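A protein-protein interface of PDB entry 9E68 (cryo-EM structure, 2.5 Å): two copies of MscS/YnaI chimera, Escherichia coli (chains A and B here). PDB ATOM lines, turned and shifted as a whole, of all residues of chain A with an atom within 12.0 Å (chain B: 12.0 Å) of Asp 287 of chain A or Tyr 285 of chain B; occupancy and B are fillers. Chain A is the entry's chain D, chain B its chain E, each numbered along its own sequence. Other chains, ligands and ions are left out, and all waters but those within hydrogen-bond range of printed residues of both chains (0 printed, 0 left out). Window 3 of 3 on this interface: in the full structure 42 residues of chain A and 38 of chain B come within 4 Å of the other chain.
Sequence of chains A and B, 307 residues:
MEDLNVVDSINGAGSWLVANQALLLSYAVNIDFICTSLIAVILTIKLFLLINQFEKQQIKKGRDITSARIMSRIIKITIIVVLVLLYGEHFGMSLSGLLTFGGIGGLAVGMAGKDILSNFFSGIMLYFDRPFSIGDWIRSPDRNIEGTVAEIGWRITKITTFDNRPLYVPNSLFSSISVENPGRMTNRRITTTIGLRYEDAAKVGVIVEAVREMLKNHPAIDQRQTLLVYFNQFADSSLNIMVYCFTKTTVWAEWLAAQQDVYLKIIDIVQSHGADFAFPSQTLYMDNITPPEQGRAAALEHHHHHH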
ATOM      1  N   THR A 283      11.925  22.461 -21.953  1.00  0.00           N
ATOM      2  CA  THR A 283      11.147  21.228 -21.916  1.00  0.00           C
ATOM      3  C   THR A 283       9.800  21.508 -21.258  1.00  0.00           C
ATOM      4  O   THR A 283       9.621  22.536 -20.598  1.00  0.00           O
ATOM      5  CB  THR A 283      11.867  20.096 -21.166  1.00  0.00           C
ATOM      6  OG1 THR A 283      11.605  20.201 -19.765  1.00  0.00           O
ATOM      7  CG2 THR A 283      13.368  20.153 -21.402  1.00  0.00           C
ATOM      8  N   LEU A 284       8.852  20.585 -21.431  1.00  0.00           N
ATOM      9  CA  LEU A 284       7.447  20.883 -21.174  1.00  0.00           C
ATOM     10  C   LEU A 284       6.805  20.054 -20.070  1.00  0.00           C
ATOM     11  O   LEU A 284       6.017  20.600 -19.293  1.00  0.00           O
ATOM     12  CB  LEU A 284       6.642  20.724 -22.470  1.00  0.00           C
ATOM     13  CG  LEU A 284       6.953  21.771 -23.539  1.00  0.00           C
ATOM     14  CD1 LEU A 284       5.962  21.671 -24.683  1.00  0.00           C
ATOM     15  CD2 LEU A 284       6.948  23.167 -22.937  1.00  0.00           C
ATOM     16  N   TYR A 285       7.084  18.749 -19.989  1.00  0.00           N
ATOM     17  CA  TYR A 285       6.477  17.905 -18.956  1.00  0.00           C
ATOM     18  C   TYR A 285       4.954  17.995 -18.939  1.00  0.00           C
ATOM     19  O   TYR A 285       4.383  18.594 -18.022  1.00  0.00           O
ATOM     20  CB  TYR A 285       7.011  18.261 -17.564  1.00  0.00           C
ATOM     21  CG  TYR A 285       8.426  17.807 -17.282  1.00  0.00           C
ATOM     22  CD1 TYR A 285       8.752  16.459 -17.275  1.00  0.00           C
ATOM     23  CD2 TYR A 285       9.426  18.724 -16.989  1.00  0.00           C
ATOM     24  CE1 TYR A 285      10.039  16.037 -17.009  1.00  0.00           C
ATOM     25  CE2 TYR A 285      10.717  18.311 -16.720  1.00  0.00           C
ATOM     26  CZ  TYR A 285      11.017  16.967 -16.731  1.00  0.00           C
ATOM     27  OH  TYR A 285      12.302  16.554 -16.464  1.00  0.00           O
ATOM     28  N   MET A 286       4.284  17.425 -19.939  1.00  0.00           N
ATOM     29  CA  MET A 286       2.834  17.557 -20.049  1.00  0.00           C
ATOM     30  C   MET A 286       2.127  16.933 -18.852  1.00  0.00           C
ATOM     31  O   MET A 286       2.664  16.047 -18.181  1.00  0.00           O
ATOM     32  CB  MET A 286       2.307  16.887 -21.316  1.00  0.00           C
ATOM     33  CG  MET A 286       2.393  17.716 -22.576  1.00  0.00           C
ATOM     34  SD  MET A 286       2.499  16.622 -24.003  1.00  0.00           S
ATOM     35  CE  MET A 286       3.522  15.306 -23.345  1.00  0.00           C
ATOM     36  N   ASP A 287       0.914  17.409 -18.592  1.00  0.00           N
ATOM     37  CA  ASP A 287       0.030  16.791 -17.612  1.00  0.00           C
ATOM     38  C   ASP A 287      -1.407  17.117 -18.012  1.00  0.00           C
ATOM     39  O   ASP A 287      -2.166  16.233 -18.412  1.00  0.00           O
ATOM     40  CB  ASP A 287       0.348  17.286 -16.195  1.00  0.00           C
ATOM     41  CG  ASP A 287      -0.547  16.664 -15.125  1.00  0.00           C
ATOM     42  OD1 ASP A 287      -1.745  16.407 -15.371  1.00  0.00           O
ATOM     43  OD2 ASP A 287      -0.033  16.416 -14.014  1.00  0.00           O
ATOM     44  N   SER B 281      12.207  23.875 -18.298  1.00  0.00           N
ATOM     45  CA  SER B 281      11.471  22.699 -17.831  1.00  0.00           C
ATOM     46  C   SER B 281      10.328  23.071 -16.877  1.00  0.00           C
ATOM     47  O   SER B 281      10.332  22.737 -15.692  1.00  0.00           O
ATOM     48  CB  SER B 281      12.429  21.705 -17.165  1.00  0.00           C
ATOM     49  OG  SER B 281      12.573  21.986 -15.785  1.00  0.00           O
ATOM     50  N   GLN B 282       9.342  23.776 -17.427  1.00  0.00           N
ATOM     51  CA  GLN B 282       8.105  24.023 -16.702  1.00  0.00           C
ATOM     52  C   GLN B 282       7.139  22.856 -16.919  1.00  0.00           C
ATOM     53  O   GLN B 282       7.499  21.821 -17.481  1.00  0.00           O
ATOM     54  CB  GLN B 282       7.486  25.350 -17.137  1.00  0.00           C
ATOM     55  CG  GLN B 282       6.925  25.352 -18.548  1.00  0.00           C
ATOM     56  CD  GLN B 282       6.860  26.744 -19.142  1.00  0.00           C
ATOM     57  OE1 GLN B 282       6.142  27.611 -18.643  1.00  0.00           O
ATOM     58  NE2 GLN B 282       7.611  26.967 -20.213  1.00  0.00           N
ATOM     59  N   THR B 283       5.902  23.006 -16.440  1.00  0.00           N
ATOM     60  CA  THR B 283       4.827  22.062 -16.720  1.00  0.00           C
ATOM     61  C   THR B 283       3.645  22.814 -17.318  1.00  0.00           C
ATOM     62  O   THR B 283       3.594  24.047 -17.276  1.00  0.00           O
ATOM     63  CB  THR B 283       4.374  21.292 -15.469  1.00  0.00           C
ATOM     64  OG1 THR B 283       3.345  22.024 -14.797  1.00  0.00           O
ATOM     65  CG2 THR B 283       5.535  21.071 -14.517  1.00  0.00           C
ATOM     66  N   LEU B 284       2.687  22.069 -17.872  1.00  0.00           N
ATOM     67  CA  LEU B 284       1.693  22.653 -18.765  1.00  0.00           C
ATOM     68  C   LEU B 284       0.259  22.574 -18.260  1.00  0.00           C
ATOM     69  O   LEU B 284      -0.489  23.541 -18.425  1.00  0.00           O
ATOM     70  CB  LEU B 284       1.791  21.990 -20.145  1.00  0.00           C
ATOM     71  CG  LEU B 284       3.078  22.306 -20.907  1.00  0.00           C
ATOM     72  CD1 LEU B 284       3.002  21.790 -22.334  1.00  0.00           C
ATOM     73  CD2 LEU B 284       3.359  23.801 -20.887  1.00  0.00           C
ATOM     74  N   TYR B 285      -0.162  21.448 -17.675  1.00  0.00           N
ATOM     75  CA  TYR B 285      -1.545  21.287 -17.227  1.00  0.00           C
ATOM     76  C   TYR B 285      -2.546  21.619 -18.330  1.00  0.00           C
ATOM     77  O   TYR B 285      -3.282  22.603 -18.223  1.00  0.00           O
ATOM     78  CB  TYR B 285      -1.838  22.160 -16.001  1.00  0.00           C
ATOM     79  CG  TYR B 285      -1.200  21.689 -14.717  1.00  0.00           C
ATOM     80  CD1 TYR B 285      -1.603  20.506 -14.113  1.00  0.00           C
ATOM     81  CD2 TYR B 285      -0.213  22.438 -14.093  1.00  0.00           C
ATOM     82  CE1 TYR B 285      -1.029  20.074 -12.935  1.00  0.00           C
ATOM     83  CE2 TYR B 285       0.366  22.015 -12.913  1.00  0.00           C
ATOM     84  CZ  TYR B 285      -0.045  20.832 -12.339  1.00  0.00           C
ATOM     85  OH  TYR B 285       0.528  20.406 -11.165  1.00  0.00           O
ATOM     86  N   MET B 286      -2.577  20.815 -19.390  1.00  0.00           N
ATOM     87  CA  MET B 286      -3.416  21.113 -20.543  1.00  0.00           C
ATOM     88  C   MET B 286      -4.892  21.069 -20.171  1.00  0.00           C
ATOM     89  O   MET B 286      -5.293  20.368 -19.238  1.00  0.00           O
ATOM     90  CB  MET B 286      -3.147  20.124 -21.676  1.00  0.00           C
ATOM     91  CG  MET B 286      -2.093  20.576 -22.666  1.00  0.00           C
ATOM     92  SD  MET B 286      -1.331  19.172 -23.497  1.00  0.00           S
ATOM     93  CE  MET B 286      -1.106  18.058 -22.114  1.00  0.00           C
ATOM     94  N   ASP B 287      -5.697  21.827 -20.908  1.00  0.00           N
ATOM     95  CA  ASP B 287      -7.143  21.823 -20.720  1.00  0.00           C
ATOM     96  C   ASP B 287      -7.803  22.119 -22.063  1.00  0.00           C
ATOM     97  O   ASP B 287      -8.584  21.316 -22.572  1.00  0.00           O
ATOM     98  CB  ASP B 287      -7.552  22.848 -19.654  1.00  0.00           C
ATOM     99  CG  ASP B 287      -9.057  22.874 -19.386  1.00  0.00           C
ATOM    100  OD1 ASP B 287      -9.432  23.074 -18.212  1.00  0.00           O
ATOM    101  OD2 ASP B 287      -9.869  22.707 -20.321  1.00  0.00           O
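Of the 7 printed residues of chain B, 6 touch a printed residue of chain A.
Hydrophobic or aromatic side chains of chain B within 4 Å of the printed part of chain A: Leu 284, Tyr 285 and Met 286.
Printed residues of chain A that touch a printed residue of chain B: Thr 283, Leu 284, Tyr 285, Met 286 and Asp 287.
Hydrophobic or aromatic side chains of chain A within 4 Å of the printed part of chain B: Leu 284, Tyr 285 and Met 286.
Among the printed residues, 11 pairs touch across the chains.
The backbone NH of Gln 282 of chain B is in hydrogen-bond range of the backbone carbonyl oxygen of Thr 283 of chain A, 3.4 Å away.
The backbone carbonyl oxygen (O) of Gln 282 of chain B lies close to the backbone carbonyl oxygen (O) of Leu 284 of chain A (2.6 Å).
Ser 281 of chain B touches Thr 283 of chain A.
Thr 283 of chain B touches Leu 284 of chain A (CA to O, 3.2 Å).
CG of Leu 284 of chain B touches O of Leu 284 of chain A (3.8 Å).
Ser 281 of chain B touches Tyr 285 of chain A.
Gln 282 of chain B touches Tyr 285 of chain A (O to CB, 3.6 Å).
Tyr 285 of chain A touches Thr 283 of chain B.
Tyr 285 of chain A touches Leu 284 of chain B.
Met 286 of chain B touches Met 286 of chain A.
Asp 287 of chain A touches Tyr 285 of chain B (OD2 to CE1, 3.9 Å).
Asp 287 of chain A touches just one residue of chain B: Tyr 285 (3.9 Å).
Of the printed residues of chain A, Tyr 285 of chain B touches Asp 287 (3.9 Å).
Of the printed residues of chain A, Thr 283 of chain B touches Leu 284 (3.2 Å) and Tyr 285 (3.7 Å).
Leu 284 of chain B touches two residues of chain A.
Met 286 of chain B touches just one residue of chain A: Met 286 (3.5 Å).
No residue of chain A comes within 4 Å of Asp 287 of chain B.
Of the printed residues of chain B, Leu 284 of chain A touches Gln 282, Thr 283 and Leu 284.
Printed residues of chain A within 4 Å of Ser 281 of chain B: Thr 283 and Tyr 285.
Of the printed residues of chain B, Thr 283 of chain A touches Ser 281 and Gln 282.
The nearest residue of chain A that does not touch Tyr 285 of chain B is Met 286 of chain A (5.2 Å).
Leu 284 of chain A touches Thr 283 of chain B, but with the chains exchanged Thr 283 of chain A does not touch Leu 284 of chain B (6.4 Å).
Tyr 285 of chain A touches Thr 283 of chain B, but with the chains exchanged Thr 283 of chain A does not touch Tyr 285 of chain B (10.3 Å).
Met 286 of chain B touches its own counterpart, Met 286 of chain A.
Asp 287 of chain A touches Tyr 285 of chain B, but with the chains exchanged Tyr 285 of chain A does not touch Asp 287 of chain B (11.0 Å).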
